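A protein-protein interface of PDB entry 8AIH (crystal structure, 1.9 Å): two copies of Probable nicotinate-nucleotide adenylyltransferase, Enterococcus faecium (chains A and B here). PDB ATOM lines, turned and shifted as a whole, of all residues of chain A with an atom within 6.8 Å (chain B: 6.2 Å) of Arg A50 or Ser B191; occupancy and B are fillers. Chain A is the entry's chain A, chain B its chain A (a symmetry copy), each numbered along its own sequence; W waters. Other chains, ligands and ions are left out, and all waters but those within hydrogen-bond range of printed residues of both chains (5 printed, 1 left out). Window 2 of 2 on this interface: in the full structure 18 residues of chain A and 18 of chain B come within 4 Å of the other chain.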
ATOM      1  N   ALA A  45      15.735  -4.344 -17.075  1.00  0.00           N
ATOM      2  CA  ALA A  45      14.922  -4.248 -18.269  1.00  0.00           C
ATOM      3  C   ALA A  45      14.787  -2.801 -18.725  1.00  0.00           C
ATOM      4  O   ALA A  45      14.742  -2.540 -19.920  1.00  0.00           O
ATOM      5  CB  ALA A  45      13.549  -4.860 -18.025  1.00  0.00           C
ATOM      6  N   GLU A  46      14.775  -1.851 -17.806  1.00  0.00           N
ATOM      7  CA  GLU A  46      14.561  -0.473 -18.224  1.00  0.00           C
ATOM      8  C   GLU A  46      15.817   0.158 -18.786  1.00  0.00           C
ATOM      9  O   GLU A  46      15.741   0.897 -19.780  1.00  0.00           O
ATOM     10  CB  GLU A  46      13.998   0.366 -17.062  1.00  0.00           C
ATOM     11  CG  GLU A  46      13.724   1.870 -17.402  1.00  0.00           C
ATOM     12  CD  GLU A  46      12.358   2.026 -17.896  1.00  0.00           C
ATOM     13  OE1 GLU A  46      11.645   1.047 -17.580  1.00  0.00           O
ATOM     14  OE2 GLU A  46      11.967   3.103 -18.482  1.00  0.00           O
ATOM     15  N   GLN A  47      16.959  -0.149 -18.158  1.00  0.00           N
ATOM     16  CA  GLN A  47      18.263   0.377 -18.568  1.00  0.00           C
ATOM     17  C   GLN A  47      18.704  -0.207 -19.903  1.00  0.00           C
ATOM     18  O   GLN A  47      19.110   0.535 -20.802  1.00  0.00           O
ATOM     19  CB  GLN A  47      19.344   0.078 -17.517  1.00  0.00           C
ATOM     20  CG  GLN A  47      19.313   0.931 -16.238  1.00  0.00           C
ATOM     21  CD  GLN A  47      19.858   2.334 -16.430  1.00  0.00           C
ATOM     22  OE1 GLN A  47      21.026   2.537 -16.832  1.00  0.00           O
ATOM     23  NE2 GLN A  47      19.009   3.323 -16.182  1.00  0.00           N
ATOM     24  N   ALA A  48      18.686  -1.540 -20.032  1.00  0.00           N
ATOM     25  CA  ALA A  48      18.975  -2.168 -21.327  1.00  0.00           C
ATOM     26  C   ALA A  48      18.146  -1.540 -22.450  1.00  0.00           C
ATOM     27  O   ALA A  48      18.697  -1.036 -23.438  1.00  0.00           O
ATOM     28  CB  ALA A  48      18.774  -3.701 -21.250  1.00  0.00           C
ATOM     29  N   GLY A  49      16.824  -1.467 -22.285  1.00  0.00           N
ATOM     30  CA  GLY A  49      16.005  -1.038 -23.390  1.00  0.00           C
ATOM     31  C   GLY A  49      16.174   0.439 -23.672  1.00  0.00           C
ATOM     32  O   GLY A  49      16.236   0.853 -24.832  1.00  0.00           O
ATOM     33  N   ARG A  50      16.238   1.269 -22.616  1.00  0.00           N
ATOM     34  CA  ARG A  50      16.325   2.719 -22.810  1.00  0.00           C
ATOM     35  C   ARG A  50      17.712   3.124 -23.282  1.00  0.00           C
ATOM     36  O   ARG A  50      17.867   4.069 -24.055  1.00  0.00           O
ATOM     37  CB  ARG A  50      16.003   3.445 -21.512  1.00  0.00           C
ATOM     38  CG  ARG A  50      14.540   3.362 -21.072  1.00  0.00           C
ATOM     39  CD  ARG A  50      13.690   4.139 -22.048  1.00  0.00           C
ATOM     40  NE  ARG A  50      12.382   4.356 -21.462  1.00  0.00           N
ATOM     41  CZ  ARG A  50      11.351   4.878 -22.109  1.00  0.00           C
ATOM     42  NH1 ARG A  50      11.447   5.233 -23.380  1.00  0.00           N
ATOM     43  NH2 ARG A  50      10.190   5.030 -21.466  1.00  0.00           N
ATOM     44  N   ASN A  51      18.749   2.448 -22.802  1.00  0.00           N
ATOM     45  CA  ASN A  51      20.070   2.905 -23.211  1.00  0.00           C
ATOM     46  C   ASN A  51      20.336   2.604 -24.680  1.00  0.00           C
ATOM     47  O   ASN A  51      21.001   3.398 -25.350  1.00  0.00           O
ATOM     48  CB  ASN A  51      21.123   2.308 -22.292  1.00  0.00           C
ATOM     49  CG  ASN A  51      21.027   2.862 -20.869  1.00  0.00           C
ATOM     50  OD1 ASN A  51      20.544   3.979 -20.670  1.00  0.00           O
ATOM     51  ND2 ASN A  51      21.496   2.096 -19.881  1.00  0.00           N
ATOM     52  N   LEU A  52      19.832   1.483 -25.189  1.00  0.00           N
ATOM     53  CA  LEU A  52      19.938   1.118 -26.596  1.00  0.00           C
ATOM     54  C   LEU A  52      18.943   1.883 -27.470  1.00  0.00           C
ATOM     55  O   LEU A  52      19.126   1.947 -28.688  1.00  0.00           O
ATOM     56  CB  LEU A  52      19.703  -0.388 -26.753  1.00  0.00           C
ATOM     57  CG  LEU A  52      20.823  -1.359 -26.332  1.00  0.00           C
ATOM     58  CD1 LEU A  52      20.425  -2.867 -26.424  1.00  0.00           C
ATOM     59  CD2 LEU A  52      22.107  -1.071 -27.045  1.00  0.00           C
ATOM     60  N   GLY A  53      17.907   2.480 -26.879  1.00  0.00           N
ATOM     61  CA  GLY A  53      16.861   3.096 -27.659  1.00  0.00           C
ATOM     62  C   GLY A  53      15.782   2.166 -28.177  1.00  0.00           C
ATOM     63  O   GLY A  53      15.164   2.483 -29.199  1.00  0.00           O
ATOM     64  N   LEU A  54      15.537   1.031 -27.513  1.00  0.00           N
ATOM     65  CA  LEU A  54      14.517   0.093 -27.952  1.00  0.00           C
ATOM     66  C   LEU A  54      13.133   0.702 -27.722  1.00  0.00           C
ATOM     67  O   LEU A  54      12.979   1.659 -26.976  1.00  0.00           O
ATOM     68  CB  LEU A  54      14.539  -1.195 -27.135  1.00  0.00           C
ATOM     69  CG  LEU A  54      15.909  -1.912 -27.123  1.00  0.00           C
ATOM     70  CD1 LEU A  54      15.791  -3.171 -26.300  1.00  0.00           C
ATOM     71  CD2 LEU A  54      16.248  -2.225 -28.536  1.00  0.00           C
ATOM     72  N   ASP A  55      12.131   0.120 -28.392  1.00  0.00           N
ATOM     73  CA  ASP A  55      10.748   0.660 -28.247  1.00  0.00           C
ATOM     74  C   ASP A  55      10.027   0.046 -27.043  1.00  0.00           C
ATOM     75  O   ASP A  55       9.106   0.656 -26.481  1.00  0.00           O
ATOM     76  CB  ASP A  55       9.916   0.449 -29.529  1.00  0.00           C
ATOM     77  CG  ASP A  55      10.539   1.070 -30.794  1.00  0.00           C
ATOM     78  OD1 ASP A  55      10.959   2.269 -30.786  1.00  0.00           O
ATOM     79  OD2 ASP A  55      10.516   0.369 -31.818  1.00  0.00           O
ATOM     80  N   VAL A  57      10.489  -3.247 -23.666  1.00  0.00           N
ATOM     81  CA  VAL A  57      11.085  -4.476 -23.124  1.00  0.00           C
ATOM     82  C   VAL A  57       9.969  -5.305 -22.513  1.00  0.00           C
ATOM     83  O   VAL A  57       9.027  -4.770 -21.904  1.00  0.00           O
ATOM     84  CB  VAL A  57      12.161  -4.151 -22.091  1.00  0.00           C
ATOM     85  CG1 VAL A  57      12.907  -5.511 -21.595  1.00  0.00           C
ATOM     86  CG2 VAL A  57      13.112  -3.166 -22.715  1.00  0.00           C
ATOM     87  N   ASN A  90       4.203   1.771 -15.916  1.00  0.00           N
ATOM     88  CA  ASN A  90       5.311   1.952 -16.856  1.00  0.00           C
ATOM     89  C   ASN A  90       4.933   1.435 -18.230  1.00  0.00           C
ATOM     90  O   ASN A  90       5.074   0.235 -18.492  1.00  0.00           O
ATOM     91  CB  ASN A  90       6.542   1.209 -16.310  1.00  0.00           C
ATOM     92  CG  ASN A  90       7.788   1.469 -17.111  1.00  0.00           C
ATOM     93  OD1 ASN A  90       7.739   2.117 -18.160  1.00  0.00           O
ATOM     94  ND2 ASN A  90       8.944   0.931 -16.639  1.00  0.00           N
ATOM     95  N   PRO A  91       4.512   2.287 -19.162  1.00  0.00           N
ATOM     96  CA  PRO A  91       4.148   1.785 -20.495  1.00  0.00           C
ATOM     97  C   PRO A  91       5.291   1.157 -21.232  1.00  0.00           C
ATOM     98  O   PRO A  91       5.068   0.566 -22.293  1.00  0.00           O
ATOM     99  CB  PRO A  91       3.735   3.030 -21.252  1.00  0.00           C
ATOM    100  CG  PRO A  91       4.397   4.133 -20.507  1.00  0.00           C
ATOM    101  CD  PRO A  91       4.398   3.751 -19.091  1.00  0.00           C
ATOM    102  N   PHE A  92       6.507   1.319 -20.739  1.00  0.00           N
ATOM    103  CA  PHE A  92       7.675   0.865 -21.478  1.00  0.00           C
ATOM    104  C   PHE A  92       8.072  -0.558 -21.160  1.00  0.00           C
ATOM    105  O   PHE A  92       8.838  -1.145 -21.959  1.00  0.00           O
ATOM    106  CB  PHE A  92       8.848   1.794 -21.155  1.00  0.00           C
ATOM    107  CG  PHE A  92      10.119   1.454 -21.905  1.00  0.00           C
ATOM    108  CD1 PHE A  92      10.324   1.837 -23.242  1.00  0.00           C
ATOM    109  CD2 PHE A  92      11.113   0.727 -21.253  1.00  0.00           C
ATOM    110  CE1 PHE A  92      11.534   1.488 -23.926  1.00  0.00           C
ATOM    111  CE2 PHE A  92      12.312   0.413 -21.918  1.00  0.00           C
ATOM    112  CZ  PHE A  92      12.530   0.784 -23.229  1.00  0.00           C
ATOM    113  N   VAL A 170      25.556  -3.674 -23.348  1.00  0.00           N
ATOM    114  CA  VAL A 170      25.006  -2.431 -22.807  1.00  0.00           C
ATOM    115  C   VAL A 170      25.279  -2.368 -21.310  1.00  0.00           C
ATOM    116  O   VAL A 170      25.223  -3.386 -20.615  1.00  0.00           O
ATOM    117  CB  VAL A 170      23.492  -2.341 -23.083  1.00  0.00           C
ATOM    118  CG1 VAL A 170      22.786  -3.456 -22.372  1.00  0.00           C
ATOM    119  CG2 VAL A 170      22.939  -0.995 -22.627  1.00  0.00           C
ATOM    120  N   LYS B 185      23.870  10.850 -15.969  1.00  0.00           N
ATOM    121  CA  LYS B 185      22.720  10.301 -16.678  1.00  0.00           C
ATOM    122  C   LYS B 185      21.674  11.384 -16.889  1.00  0.00           C
ATOM    123  O   LYS B 185      21.178  11.565 -18.008  1.00  0.00           O
ATOM    124  CB  LYS B 185      22.134   9.116 -15.910  1.00  0.00           C
ATOM    125  CG  LYS B 185      22.954   7.857 -16.054  1.00  0.00           C
ATOM    126  CD  LYS B 185      22.277   6.671 -15.418  1.00  0.00           C
ATOM    127  CE  LYS B 185      23.042   5.356 -15.706  1.00  0.00           C
ATOM    128  NZ  LYS B 185      23.225   4.973 -17.127  1.00  0.00           N
ATOM    129  N   GLY B 189      20.478  13.071 -20.371  1.00  0.00           N
ATOM    130  CA  GLY B 189      19.144  12.697 -20.794  1.00  0.00           C
ATOM    131  C   GLY B 189      18.892  11.209 -20.764  1.00  0.00           C
ATOM    132  O   GLY B 189      18.060  10.705 -21.525  1.00  0.00           O
ATOM    133  N   CYS B 190      19.651  10.497 -19.946  1.00  0.00           N
ATOM    134  CA  CYS B 190      19.484   9.032 -19.841  1.00  0.00           C
ATOM    135  C   CYS B 190      18.440   8.699 -18.764  1.00  0.00           C
ATOM    136  O   CYS B 190      18.204   9.520 -17.891  1.00  0.00           O
ATOM    137  CB  CYS B 190      20.830   8.387 -19.547  1.00  0.00           C
ATOM    138  SG  CYS B 190      22.071   8.696 -20.830  1.00  0.00           S
ATOM    139  N   SER B 191      17.805   7.540 -18.880  1.00  0.00           N
ATOM    140  CA  SER B 191      16.799   7.105 -17.919  1.00  0.00           C
ATOM    141  C   SER B 191      17.415   6.941 -16.537  1.00  0.00           C
ATOM    142  O   SER B 191      18.529   6.427 -16.404  1.00  0.00           O
ATOM    143  CB  SER B 191      16.173   5.785 -18.375  1.00  0.00           C
ATOM    144  OG  SER B 191      15.121   5.376 -17.493  1.00  0.00           O
ATOM    145  N   ILE B 192      16.683   7.365 -15.499  1.00  0.00           N
ATOM    146  CA  ILE B 192      17.043   7.005 -14.122  1.00  0.00           C
ATOM    147  C   ILE B 192      15.895   6.310 -13.393  1.00  0.00           C
ATOM    148  O   ILE B 192      15.894   6.230 -12.154  1.00  0.00           O
ATOM    149  CB  ILE B 192      17.510   8.220 -13.303  1.00  0.00           C
ATOM    150  CG1 ILE B 192      16.342   9.221 -13.115  1.00  0.00           C
ATOM    151  CG2 ILE B 192      18.736   8.856 -13.960  1.00  0.00           C
ATOM    152  CD1 ILE B 192      16.651  10.478 -12.297  1.00  0.00           C
ATOM    153  N   ARG B 193      14.926   5.788 -14.142  1.00  0.00           N
ATOM    154  CA  ARG B 193      13.794   5.149 -13.484  1.00  0.00           C
ATOM    155  C   ARG B 193      14.280   3.923 -12.718  1.00  0.00           C
ATOM    156  O   ARG B 193      15.108   3.164 -13.228  1.00  0.00           O
ATOM    157  CB  ARG B 193      12.732   4.746 -14.497  1.00  0.00           C
ATOM    158  CG  ARG B 193      11.346   4.701 -13.855  1.00  0.00           C
ATOM    159  CD  ARG B 193      10.350   4.012 -14.743  1.00  0.00           C
ATOM    160  NE  ARG B 193       9.023   4.011 -14.146  1.00  0.00           N
ATOM    161  CZ  ARG B 193       7.959   4.559 -14.715  1.00  0.00           C
ATOM    162  NH1 ARG B 193       8.042   5.173 -15.887  1.00  0.00           N
ATOM    163  NH2 ARG B 193       6.789   4.494 -14.090  1.00  0.00           N
ATOM    164  N   LEU B 195      16.321   3.551 -10.449  1.00  0.00           N
ATOM    165  CA  LEU B 195      17.580   3.929  -9.797  1.00  0.00           C
ATOM    166  C   LEU B 195      17.356   4.952  -8.692  1.00  0.00           C
ATOM    167  O   LEU B 195      18.098   4.972  -7.691  1.00  0.00           O
ATOM    168  CB  LEU B 195      18.552   4.523 -10.837  1.00  0.00           C
ATOM    169  CG  LEU B 195      18.963   3.653 -12.046  1.00  0.00           C
ATOM    170  CD1 LEU B 195      19.836   4.412 -13.059  1.00  0.00           C
ATOM    171  CD2 LEU B 195      19.576   2.280 -11.660  1.00  0.00           C
HETATM  172  O   HOH W   1       9.702   4.223 -18.722  1.00  0.00           O
HETATM  173  O   HOH W   2      16.521   2.988 -15.557  1.00  0.00           O
HETATM  174  O   HOH W   3      12.660   6.219 -18.246  1.00  0.00           O
HETATM  175  O   HOH W   4      18.698   5.957 -21.188  1.00  0.00           O
HETATM  176  O   HOH W   5      24.178   2.702 -17.088  1.00  0.00           O
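Printed residues of chain A that touch a printed residue of chain B: Glu A46, Gln A47, Arg A50 and Asn A90. Of the 7 printed residues of chain B, 4 touch a printed residue of chain A. Among the printed residues, 6 pairs touch across the chains.
The guanidinium group (NE) of Arg A50 lies within salt-bridge range of the side-chain carboxylate (OE2) of Glu A46 (3.3 Å). ND2 of Asn A90 is in hydrogen-bond range of OE1 of Glu A46, at 2.9 Å. The backbone carbonyl oxygen of Gln A47 sits at hydrogen-bond distance from the side-chain amide nitrogen of Asn A51. OD1 of Asn A90 sits close to N of Phe A92 (3.0 Å). The backbone carbonyl oxygen (O) of Lys B185 lies within hydrogen-bond range of the backbone NH (N) of Cys B190 (2.7 Å). N of Arg B193 lies within hydrogen-bond range of OG of Ser B191, 3.4 Å away.
Glu A46 touches Ser B191. Leu B195 touches Gln A47. Arg A50 touches Ser B191. Arg B193 touches Asn A90.
No position is printed for both chains.
Of chain A, only Glu A46 (3.8 Å), Gln A47 (3.1 Å) and Arg A50 (3.9 Å) come within 4 Å of Ser B191. Printed residues of chain B within 4 Å of Gln A47: Lys B185 (3.3 Å), Ser B191 (3.1 Å) and Leu B195 (3.4 Å). Printed residues of chain A within 4 Å of Arg B193: Asn A90 (3.8 Å). Asp A55 touches none of the printed residues of chain B. The nearest residue of chain B that does not touch Arg A50 is Arg B193 (6.0 Å). The nearest residue of chain A that does not touch Ser B191 is Asn A51 (4.8 Å). The nearest printed residue of chain B that does not touch Glu A46 is Arg B193 (4.2 Å).
OE1 of Gln A47 is in hydrogen-bond range of NZ of Lys B185, at 3.3 Å. The side-chain amide nitrogen (NE2) of Gln A47 is in hydrogen-bond range of the backbone carbonyl oxygen (O) of Ser B191, 3.1 Å away.
Water W5 lies within hydrogen-bond range of the side-chain amino group of Lys B185 (2.5 Å) and the side-chain amide oxygen of Gln A47 (3.2 Å). Water W1 lies within hydrogen-bond range of the side-chain carboxylate (OE2) of Glu A46 (2.5 Å), the guanidinium group (NH2) of Arg A50 (2.9 Å), the side-chain amide oxygen (OD1) of Asn A90 (2.9 Å) and the guanidinium group (NH1) of Arg B193 (3.4 Å). Water W2 lies within hydrogen-bond range of NE2 of Gln A47, O of Arg B193 and OG of Ser B191. Water W3 lies within hydrogen-bond range of OG of Ser B191 and OE2 of Glu A46. Water W4 bridges the side-chain amide oxygen (OD1) of Asn A51 (2.8 Å) and the backbone NH (N) of Ser B191 (2.9 Å).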
